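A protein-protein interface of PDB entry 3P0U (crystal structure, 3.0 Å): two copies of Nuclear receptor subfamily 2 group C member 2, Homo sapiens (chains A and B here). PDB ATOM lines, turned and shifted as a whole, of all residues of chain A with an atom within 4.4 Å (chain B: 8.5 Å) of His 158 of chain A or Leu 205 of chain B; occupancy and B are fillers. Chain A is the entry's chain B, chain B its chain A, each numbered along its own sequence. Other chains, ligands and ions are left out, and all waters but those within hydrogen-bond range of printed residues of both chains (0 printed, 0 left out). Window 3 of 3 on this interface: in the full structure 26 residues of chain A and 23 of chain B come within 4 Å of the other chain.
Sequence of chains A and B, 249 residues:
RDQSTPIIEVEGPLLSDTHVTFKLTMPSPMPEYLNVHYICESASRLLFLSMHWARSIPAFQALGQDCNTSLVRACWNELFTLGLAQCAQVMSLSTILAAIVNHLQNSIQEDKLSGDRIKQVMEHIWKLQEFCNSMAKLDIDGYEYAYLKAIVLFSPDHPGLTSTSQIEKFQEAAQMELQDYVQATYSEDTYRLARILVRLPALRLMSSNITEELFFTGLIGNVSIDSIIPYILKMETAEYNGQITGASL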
ATOM      1  N   ALA A  74      14.107   5.381 -18.420  1.00  0.00           N
ATOM      2  CA  ALA A  74      14.178   4.441 -19.509  1.00  0.00           C
ATOM      3  C   ALA A  74      15.195   4.860 -20.548  1.00  0.00           C
ATOM      4  O   ALA A  74      15.418   4.131 -21.514  1.00  0.00           O
ATOM      5  CB  ALA A  74      12.815   4.304 -20.156  1.00  0.00           C
ATOM      6  N   CYS A  75      15.824   6.013 -20.380  1.00  0.00           N
ATOM      7  CA  CYS A  75      16.802   6.407 -21.356  1.00  0.00           C
ATOM      8  C   CYS A  75      17.968   7.124 -20.796  1.00  0.00           C
ATOM      9  O   CYS A  75      18.817   7.570 -21.541  1.00  0.00           O
ATOM     10  CB  CYS A  75      16.129   7.291 -22.367  1.00  0.00           C
ATOM     11  SG  CYS A  75      15.606   8.869 -21.672  1.00  0.00           S
ATOM     12  N   GLU A  78      21.273   6.684 -22.225  1.00  0.00           N
ATOM     13  CA  GLU A  78      21.386   7.297 -23.535  1.00  0.00           C
ATOM     14  C   GLU A  78      21.753   8.765 -23.401  1.00  0.00           C
ATOM     15  O   GLU A  78      22.711   9.209 -24.044  1.00  0.00           O
ATOM     16  CB  GLU A  78      20.097   7.125 -24.350  1.00  0.00           C
ATOM     17  CG  GLU A  78      20.051   5.818 -25.178  1.00  0.00           C
ATOM     18  CD  GLU A  78      18.628   5.541 -25.714  1.00  0.00           C
ATOM     19  OE1 GLU A  78      18.120   6.291 -26.603  1.00  0.00           O
ATOM     20  OE2 GLU A  78      17.993   4.574 -25.217  1.00  0.00           O
ATOM     21  N   SER A 155      11.022   9.009 -26.681  1.00  0.00           N
ATOM     22  CA  SER A 155      10.989   7.861 -27.568  1.00  0.00           C
ATOM     23  C   SER A 155       9.740   7.077 -27.249  1.00  0.00           C
ATOM     24  O   SER A 155       9.476   6.795 -26.092  1.00  0.00           O
ATOM     25  CB  SER A 155      12.234   7.002 -27.409  1.00  0.00           C
ATOM     26  OG  SER A 155      12.360   6.087 -28.485  1.00  0.00           O
ATOM     27  N   PRO A 156       8.933   6.750 -28.272  1.00  0.00           N
ATOM     28  CA  PRO A 156       7.704   6.026 -28.007  1.00  0.00           C
ATOM     29  C   PRO A 156       8.002   4.558 -27.857  1.00  0.00           C
ATOM     30  O   PRO A 156       7.161   3.783 -27.421  1.00  0.00           O
ATOM     31  CB  PRO A 156       6.884   6.284 -29.265  1.00  0.00           C
ATOM     32  CG  PRO A 156       7.444   7.488 -29.830  1.00  0.00           C
ATOM     33  CD  PRO A 156       8.895   7.334 -29.618  1.00  0.00           C
ATOM     34  N   ASP A 157       9.225   4.199 -28.230  1.00  0.00           N
ATOM     35  CA  ASP A 157       9.656   2.818 -28.311  1.00  0.00           C
ATOM     36  C   ASP A 157       9.565   2.118 -26.968  1.00  0.00           C
ATOM     37  O   ASP A 157       9.237   0.924 -26.894  1.00  0.00           O
ATOM     38  CB  ASP A 157      11.094   2.805 -28.845  1.00  0.00           C
ATOM     39  CG  ASP A 157      11.209   3.424 -30.253  1.00  0.00           C
ATOM     40  OD1 ASP A 157      12.344   3.673 -30.746  1.00  0.00           O
ATOM     41  OD2 ASP A 157      10.149   3.644 -30.885  1.00  0.00           O
ATOM     42  N   HIS A 158       9.843   2.880 -25.910  1.00  0.00           N
ATOM     43  CA  HIS A 158      10.002   2.316 -24.583  1.00  0.00           C
ATOM     44  C   HIS A 158       8.692   1.756 -24.031  1.00  0.00           C
ATOM     45  O   HIS A 158       7.644   2.348 -24.173  1.00  0.00           O
ATOM     46  CB  HIS A 158      10.622   3.347 -23.632  1.00  0.00           C
ATOM     47  CG  HIS A 158      11.942   3.857 -24.093  1.00  0.00           C
ATOM     48  ND1 HIS A 158      12.989   3.020 -24.378  1.00  0.00           N
ATOM     49  CD2 HIS A 158      12.371   5.114 -24.355  1.00  0.00           C
ATOM     50  CE1 HIS A 158      14.009   3.741 -24.810  1.00  0.00           C
ATOM     51  NE2 HIS A 158      13.663   5.016 -24.798  1.00  0.00           N
ATOM     52  N   PRO A 159       8.749   0.596 -23.394  1.00  0.00           N
ATOM     53  CA  PRO A 159       7.542   0.049 -22.797  1.00  0.00           C
ATOM     54  C   PRO A 159       7.102   0.754 -21.532  1.00  0.00           C
ATOM     55  O   PRO A 159       7.820   1.590 -21.012  1.00  0.00           O
ATOM     56  CB  PRO A 159       7.951  -1.387 -22.482  1.00  0.00           C
ATOM     57  CG  PRO A 159       8.976  -1.687 -23.489  1.00  0.00           C
ATOM     58  CD  PRO A 159       9.783  -0.432 -23.493  1.00  0.00           C
ATOM     59  N   GLY A 160       5.928   0.391 -21.039  1.00  0.00           N
ATOM     60  CA  GLY A 160       5.408   0.969 -19.794  1.00  0.00           C
ATOM     61  C   GLY A 160       5.299   2.489 -19.800  1.00  0.00           C
ATOM     62  O   GLY A 160       5.520   3.153 -18.788  1.00  0.00           O
ATOM     63  N   LEU A 161       4.960   3.045 -20.956  1.00  0.00           N
ATOM     64  CA  LEU A 161       4.818   4.488 -21.109  1.00  0.00           C
ATOM     65  C   LEU A 161       3.332   4.894 -21.207  1.00  0.00           C
ATOM     66  O   LEU A 161       2.493   4.126 -21.658  1.00  0.00           O
ATOM     67  CB  LEU A 161       5.649   4.950 -22.314  1.00  0.00           C
ATOM     68  CG  LEU A 161       6.987   5.593 -21.919  1.00  0.00           C
ATOM     69  CD1 LEU A 161       7.683   4.822 -20.833  1.00  0.00           C
ATOM     70  CD2 LEU A 161       7.883   5.749 -23.127  1.00  0.00           C
ATOM     71  N   ARG A 204      21.820   3.059 -28.509  1.00  0.00           N
ATOM     72  CA  ARG A 204      21.116   1.876 -27.992  1.00  0.00           C
ATOM     73  C   ARG A 204      21.970   0.615 -28.086  1.00  0.00           C
ATOM     74  O   ARG A 204      21.480  -0.465 -27.911  1.00  0.00           O
ATOM     75  CB  ARG A 204      19.789   1.685 -28.708  1.00  0.00           C
ATOM     76  CG  ARG A 204      18.768   2.763 -28.328  1.00  0.00           C
ATOM     77  CD  ARG A 204      17.505   2.096 -28.003  1.00  0.00           C
ATOM     78  NE  ARG A 204      16.346   2.562 -28.750  1.00  0.00           N
ATOM     79  CZ  ARG A 204      15.691   3.660 -28.447  1.00  0.00           C
ATOM     80  NH1 ARG A 204      14.616   4.020 -29.151  1.00  0.00           N
ATOM     81  NH2 ARG A 204      16.125   4.406 -27.432  1.00  0.00           N
ATOM     82  N   ASN B  77      19.167  -9.633 -36.958  1.00  0.00           N
ATOM     83  CA  ASN B  77      17.906  -9.401 -36.297  1.00  0.00           C
ATOM     84  C   ASN B  77      17.312  -8.073 -36.683  1.00  0.00           C
ATOM     85  O   ASN B  77      16.096  -7.949 -36.803  1.00  0.00           O
ATOM     86  CB  ASN B  77      18.058  -9.458 -34.784  1.00  0.00           C
ATOM     87  CG  ASN B  77      16.705  -9.450 -34.075  1.00  0.00           C
ATOM     88  OD1 ASN B  77      15.802 -10.247 -34.405  1.00  0.00           O
ATOM     89  ND2 ASN B  77      16.547  -8.531 -33.106  1.00  0.00           N
ATOM     90  N   GLU B  78      18.147  -7.071 -36.896  1.00  0.00           N
ATOM     91  CA  GLU B  78      17.629  -5.813 -37.423  1.00  0.00           C
ATOM     92  C   GLU B  78      16.999  -6.035 -38.805  1.00  0.00           C
ATOM     93  O   GLU B  78      15.814  -5.768 -39.008  1.00  0.00           O
ATOM     94  CB  GLU B  78      18.733  -4.777 -37.475  1.00  0.00           C
ATOM     95  CG  GLU B  78      19.225  -4.369 -36.090  1.00  0.00           C
ATOM     96  CD  GLU B  78      20.249  -3.211 -36.134  1.00  0.00           C
ATOM     97  OE1 GLU B  78      21.486  -3.452 -35.957  1.00  0.00           O
ATOM     98  OE2 GLU B  78      19.807  -2.050 -36.360  1.00  0.00           O
ATOM     99  N   GLU B 123       6.825  -8.010 -23.690  1.00  0.00           N
ATOM    100  CA  GLU B 123       7.387  -6.726 -24.084  1.00  0.00           C
ATOM    101  C   GLU B 123       7.997  -6.811 -25.470  1.00  0.00           C
ATOM    102  O   GLU B 123       7.789  -5.949 -26.292  1.00  0.00           O
ATOM    103  CB  GLU B 123       8.458  -6.251 -23.087  1.00  0.00           C
ATOM    104  CG  GLU B 123       7.897  -5.735 -21.763  1.00  0.00           C
ATOM    105  CD  GLU B 123       8.972  -5.185 -20.800  1.00  0.00           C
ATOM    106  OE1 GLU B 123       9.922  -5.913 -20.421  1.00  0.00           O
ATOM    107  OE2 GLU B 123       8.852  -4.016 -20.381  1.00  0.00           O
ATOM    108  N   HIS B 124       8.739  -7.869 -25.721  1.00  0.00           N
ATOM    109  CA  HIS B 124       9.418  -8.005 -26.980  1.00  0.00           C
ATOM    110  C   HIS B 124       8.438  -8.119 -28.128  1.00  0.00           C
ATOM    111  O   HIS B 124       8.578  -7.446 -29.136  1.00  0.00           O
ATOM    112  CB  HIS B 124      10.363  -9.218 -26.976  1.00  0.00           C
ATOM    113  CG  HIS B 124      11.218  -9.281 -28.192  1.00  0.00           C
ATOM    114  ND1 HIS B 124      10.767  -9.833 -29.367  1.00  0.00           N
ATOM    115  CD2 HIS B 124      12.447  -8.779 -28.447  1.00  0.00           C
ATOM    116  CE1 HIS B 124      11.695  -9.692 -30.295  1.00  0.00           C
ATOM    117  NE2 HIS B 124      12.723  -9.050 -29.762  1.00  0.00           N
ATOM    118  N   TRP B 126       5.401  -7.066 -28.006  1.00  0.00           N
ATOM    119  CA  TRP B 126       4.817  -5.748 -28.027  1.00  0.00           C
ATOM    120  C   TRP B 126       5.650  -4.805 -28.913  1.00  0.00           C
ATOM    121  O   TRP B 126       5.139  -4.226 -29.903  1.00  0.00           O
ATOM    122  CB  TRP B 126       4.710  -5.193 -26.599  1.00  0.00           C
ATOM    123  CG  TRP B 126       4.615  -3.640 -26.523  1.00  0.00           C
ATOM    124  CD1 TRP B 126       5.650  -2.733 -26.369  1.00  0.00           C
ATOM    125  CD2 TRP B 126       3.438  -2.870 -26.622  1.00  0.00           C
ATOM    126  NE1 TRP B 126       5.162  -1.456 -26.391  1.00  0.00           N
ATOM    127  CE2 TRP B 126       3.811  -1.517 -26.555  1.00  0.00           C
ATOM    128  CE3 TRP B 126       2.102  -3.194 -26.782  1.00  0.00           C
ATOM    129  CZ2 TRP B 126       2.904  -0.509 -26.616  1.00  0.00           C
ATOM    130  CZ3 TRP B 126       1.199  -2.192 -26.866  1.00  0.00           C
ATOM    131  CH2 TRP B 126       1.594  -0.854 -26.783  1.00  0.00           C
ATOM    132  N   LYS B 127       6.928  -4.648 -28.574  1.00  0.00           N
ATOM    133  CA  LYS B 127       7.771  -3.730 -29.308  1.00  0.00           C
ATOM    134  C   LYS B 127       7.761  -4.074 -30.792  1.00  0.00           C
ATOM    135  O   LYS B 127       7.774  -3.148 -31.669  1.00  0.00           O
ATOM    136  CB  LYS B 127       9.199  -3.825 -28.831  1.00  0.00           C
ATOM    137  CG  LYS B 127       9.438  -3.515 -27.376  1.00  0.00           C
ATOM    138  CD  LYS B 127      10.949  -3.466 -27.086  1.00  0.00           C
ATOM    139  CE  LYS B 127      11.312  -4.128 -25.795  1.00  0.00           C
ATOM    140  NZ  LYS B 127      12.365  -3.350 -25.045  1.00  0.00           N
ATOM    141  N   LEU B 128       7.790  -5.399 -31.042  1.00  0.00           N
ATOM    142  CA  LEU B 128       7.786  -5.983 -32.384  1.00  0.00           C
ATOM    143  C   LEU B 128       6.505  -5.593 -33.135  1.00  0.00           C
ATOM    144  O   LEU B 128       6.565  -5.178 -34.278  1.00  0.00           O
ATOM    145  CB  LEU B 128       7.915  -7.520 -32.300  1.00  0.00           C
ATOM    146  CG  LEU B 128       7.949  -8.287 -33.617  1.00  0.00           C
ATOM    147  CD1 LEU B 128       9.161  -7.831 -34.375  1.00  0.00           C
ATOM    148  CD2 LEU B 128       7.956  -9.788 -33.332  1.00  0.00           C
ATOM    149  N   GLU B 130       4.427  -3.106 -32.373  1.00  0.00           N
ATOM    150  CA  GLU B 130       4.381  -1.671 -32.394  1.00  0.00           C
ATOM    151  C   GLU B 130       5.338  -1.118 -33.465  1.00  0.00           C
ATOM    152  O   GLU B 130       5.064  -0.056 -34.033  1.00  0.00           O
ATOM    153  CB  GLU B 130       4.699  -1.143 -31.004  1.00  0.00           C
ATOM    154  CG  GLU B 130       3.734  -0.090 -30.474  1.00  0.00           C
ATOM    155  CD  GLU B 130       2.233  -0.436 -30.639  1.00  0.00           C
ATOM    156  OE1 GLU B 130       1.676  -0.182 -31.760  1.00  0.00           O
ATOM    157  OE2 GLU B 130       1.611  -0.901 -29.629  1.00  0.00           O
ATOM    158  N   ARG B 199      13.331   5.947 -36.817  1.00  0.00           N
ATOM    159  CA  ARG B 199      12.786   4.640 -36.538  1.00  0.00           C
ATOM    160  C   ARG B 199      13.881   3.604 -36.273  1.00  0.00           C
ATOM    161  O   ARG B 199      13.658   2.631 -35.556  1.00  0.00           O
ATOM    162  CB  ARG B 199      11.935   4.185 -37.726  1.00  0.00           C
ATOM    163  CG  ARG B 199      10.677   5.007 -37.913  1.00  0.00           C
ATOM    164  CD  ARG B 199       9.624   4.476 -37.018  1.00  0.00           C
ATOM    165  NE  ARG B 199       9.836   4.972 -35.684  1.00  0.00           N
ATOM    166  CZ  ARG B 199       9.742   4.242 -34.589  1.00  0.00           C
ATOM    167  NH1 ARG B 199       9.458   2.958 -34.660  1.00  0.00           N
ATOM    168  NH2 ARG B 199       9.942   4.808 -33.409  1.00  0.00           N
ATOM    169  N   LEU B 200      15.048   3.800 -36.879  1.00  0.00           N
ATOM    170  CA  LEU B 200      16.131   2.817 -36.773  1.00  0.00           C
ATOM    171  C   LEU B 200      16.540   2.482 -35.321  1.00  0.00           C
ATOM    172  O   LEU B 200      16.887   1.343 -35.018  1.00  0.00           O
ATOM    173  CB  LEU B 200      17.361   3.263 -37.576  1.00  0.00           C
ATOM    174  CG  LEU B 200      17.213   3.331 -39.103  1.00  0.00           C
ATOM    175  CD1 LEU B 200      18.419   3.998 -39.710  1.00  0.00           C
ATOM    176  CD2 LEU B 200      16.965   1.925 -39.757  1.00  0.00           C
ATOM    177  N   PRO B 201      16.477   3.459 -34.417  1.00  0.00           N
ATOM    178  CA  PRO B 201      16.889   3.157 -33.070  1.00  0.00           C
ATOM    179  C   PRO B 201      16.053   2.074 -32.485  1.00  0.00           C
ATOM    180  O   PRO B 201      16.544   1.318 -31.682  1.00  0.00           O
ATOM    181  CB  PRO B 201      16.705   4.497 -32.349  1.00  0.00           C
ATOM    182  CG  PRO B 201      17.113   5.482 -33.411  1.00  0.00           C
ATOM    183  CD  PRO B 201      16.337   4.909 -34.604  1.00  0.00           C
ATOM    184  N   ALA B 202      14.800   1.978 -32.912  1.00  0.00           N
ATOM    185  CA  ALA B 202      13.851   0.975 -32.359  1.00  0.00           C
ATOM    186  C   ALA B 202      14.308  -0.474 -32.622  1.00  0.00           C
ATOM    187  O   ALA B 202      14.094  -1.359 -31.760  1.00  0.00           O
ATOM    188  CB  ALA B 202      12.431   1.180 -32.908  1.00  0.00           C
ATOM    189  N   LEU B 203      14.920  -0.711 -33.789  1.00  0.00           N
ATOM    190  CA  LEU B 203      15.486  -2.016 -34.093  1.00  0.00           C
ATOM    191  C   LEU B 203      16.478  -2.523 -33.022  1.00  0.00           C
ATOM    192  O   LEU B 203      16.513  -3.723 -32.727  1.00  0.00           O
ATOM    193  CB  LEU B 203      16.171  -2.016 -35.465  1.00  0.00           C
ATOM    194  CG  LEU B 203      15.280  -1.861 -36.719  1.00  0.00           C
ATOM    195  CD1 LEU B 203      16.163  -1.567 -37.946  1.00  0.00           C
ATOM    196  CD2 LEU B 203      14.386  -3.065 -37.022  1.00  0.00           C
ATOM    197  N   ARG B 204      17.269  -1.635 -32.419  1.00  0.00           N
ATOM    198  CA  ARG B 204      18.259  -2.061 -31.392  1.00  0.00           C
ATOM    199  C   ARG B 204      17.600  -2.465 -30.076  1.00  0.00           C
ATOM    200  O   ARG B 204      17.972  -3.476 -29.480  1.00  0.00           O
ATOM    201  CB  ARG B 204      19.244  -0.966 -31.044  1.00  0.00           C
ATOM    202  CG  ARG B 204      19.867  -0.279 -32.215  1.00  0.00           C
ATOM    203  CD  ARG B 204      20.975  -1.045 -32.905  1.00  0.00           C
ATOM    204  NE  ARG B 204      22.062  -0.086 -33.123  1.00  0.00           N
ATOM    205  CZ  ARG B 204      22.990  -0.217 -34.046  1.00  0.00           C
ATOM    206  NH1 ARG B 204      23.932   0.702 -34.177  1.00  0.00           N
ATOM    207  NH2 ARG B 204      22.965  -1.278 -34.848  1.00  0.00           N
ATOM    208  N   LEU B 205      16.607  -1.700 -29.626  1.00  0.00           N
ATOM    209  CA  LEU B 205      15.819  -2.116 -28.451  1.00  0.00           C
ATOM    210  C   LEU B 205      15.278  -3.583 -28.423  1.00  0.00           C
ATOM    211  O   LEU B 205      14.816  -4.009 -27.390  1.00  0.00           O
ATOM    212  CB  LEU B 205      14.637  -1.145 -28.219  1.00  0.00           C
ATOM    213  CG  LEU B 205      14.773   0.029 -27.224  1.00  0.00           C
ATOM    214  CD1 LEU B 205      13.408   0.358 -26.546  1.00  0.00           C
ATOM    215  CD2 LEU B 205      15.820  -0.253 -26.174  1.00  0.00           C
ATOM    216  N   MET B 206      15.290  -4.325 -29.522  1.00  0.00           N
ATOM    217  CA  MET B 206      14.670  -5.641 -29.520  1.00  0.00           C
ATOM    218  C   MET B 206      15.730  -6.721 -29.450  1.00  0.00           C
ATOM    219  O   MET B 206      16.681  -6.677 -30.228  1.00  0.00           O
ATOM    220  CB  MET B 206      13.771  -5.835 -30.741  1.00  0.00           C
ATOM    221  CG  MET B 206      12.365  -5.328 -30.485  1.00  0.00           C
ATOM    222  SD  MET B 206      11.412  -5.389 -31.964  1.00  0.00           S
ATOM    223  CE  MET B 206      12.220  -4.129 -32.953  1.00  0.00           C
ATOM    224  N   SER B 207      15.581  -7.664 -28.514  1.00  0.00           N
ATOM    225  CA  SER B 207      16.618  -8.658 -28.244  1.00  0.00           C
ATOM    226  C   SER B 207      16.659  -9.745 -29.325  1.00  0.00           C
ATOM    227  O   SER B 207      15.649 -10.354 -29.670  1.00  0.00           O
ATOM    228  CB  SER B 207      16.404  -9.280 -26.859  1.00  0.00           C
ATOM    229  OG  SER B 207      16.943 -10.596 -26.747  1.00  0.00           O
ATOM    230  N   SER B 208      17.857  -9.991 -29.834  1.00  0.00           N
ATOM    231  CA  SER B 208      18.055 -10.986 -30.869  1.00  0.00           C
ATOM    232  C   SER B 208      17.674 -12.390 -30.400  1.00  0.00           C
ATOM    233  O   SER B 208      17.141 -13.182 -31.172  1.00  0.00           O
ATOM    234  CB  SER B 208      19.508 -10.957 -31.321  1.00  0.00           C
ATOM    235  OG  SER B 208      20.005 -12.292 -31.465  1.00  0.00           O
ATOM    236  N   ILE B 210      15.431 -13.187 -27.904  1.00  0.00           N
ATOM    237  CA  ILE B 210      13.997 -13.347 -27.772  1.00  0.00           C
ATOM    238  C   ILE B 210      13.432 -13.613 -29.154  1.00  0.00           C
ATOM    239  O   ILE B 210      12.539 -14.430 -29.328  1.00  0.00           O
ATOM    240  CB  ILE B 210      13.345 -12.157 -27.139  1.00  0.00           C
ATOM    241  CG1 ILE B 210      13.804 -12.024 -25.676  1.00  0.00           C
ATOM    242  CG2 ILE B 210      11.821 -12.297 -27.223  1.00  0.00           C
ATOM    243  CD1 ILE B 210      13.095 -10.941 -24.835  1.00  0.00           C
ATOM    244  N   THR B 211      13.995 -12.967 -30.156  1.00  0.00           N
ATOM    245  CA  THR B 211      13.513 -13.144 -31.509  1.00  0.00           C
ATOM    246  C   THR B 211      13.784 -14.527 -32.003  1.00  0.00           C
ATOM    247  O   THR B 211      12.985 -15.087 -32.741  1.00  0.00           O
ATOM    248  CB  THR B 211      14.154 -12.153 -32.489  1.00  0.00           C
ATOM    249  OG1 THR B 211      13.528 -10.862 -32.346  1.00  0.00           O
ATOM    250  CG2 THR B 211      13.996 -12.657 -33.940  1.00  0.00           C
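OE1 of Glu 78 of chain B lies within salt-bridge range of NH2 of Arg 204 of chain B (2.9 Å).
OG of Ser 155 of chain A is in hydrogen-bond range of OD1 of Asp 157 of chain A.
The side-chain carboxylate (OE1) of Glu 78 of chain A lies within salt-bridge range of the guanidinium group (NH2) of Arg 204 of chain A (2.9 Å).
OG of Ser 155 of chain A lies within hydrogen-bond range of NH1 of Arg 204 of chain A (3.1 Å).
OD1 of Asp 157 of chain A lies within salt-bridge range of NH1 of Arg 204 of chain A (2.8 Å).
O of Leu 205 of chain B lies within hydrogen-bond range of NZ of Lys 127 of chain B (3.5 Å).
Printed residues of chain B that touch a printed residue of chain A: Glu 123, Arg 199, Pro 201, Ala 202, Arg 204 and Leu 205.
OD1 of Asp 157 of chain A touches CB of Ala 202 of chain B, at 3.3 Å.
Leu 205 of chain B touches His 158 of chain A.
Pro 159 of chain A touches Glu 123 of chain B.
Arg 204 of chain A touches Arg 204 of chain B (CB to CB, 3.6 Å).
Leu 205 of chain B touches Arg 204 of chain A.
His 158 of chain A touches just one residue of chain B: Leu 205 (3.5 Å).
Of chain A, only His 158 (3.5 Å) and Arg 204 (3.3 Å) come within 4 Å of Leu 205 of chain B.
Printed residues of chain B within 4 Å of Pro 159 of chain A: Glu 123.
Of the printed residues of chain B, Asp 157 of chain A touches Arg 199 and Ala 202.
Of the printed residues of chain B, Arg 204 of chain A touches Pro 201, Arg 204 and Leu 205.
His 124 of chain B touches none of the printed residues of chain A.
The nearest residue of chain B that does not touch His 158 of chain A is Trp 126 of chain B (5.1 Å).
NH2 of Arg 199 of chain B is in salt-bridge range of OD2 of Asp 157 of chain A (2.8 Å).
The backbone carbonyl oxygen of Pro 201 of chain B sits at hydrogen-bond distance from the guanidinium group of Arg 204 of chain A, at 3.2 Å.
Arg 204 of chain A touches its own counterpart, Arg 204 of chain B.
2 positions are printed for both chains.
Of the 7 pairs that touch across the chains among the printed residues, 1 has its exchanged pair printed and touching as well.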
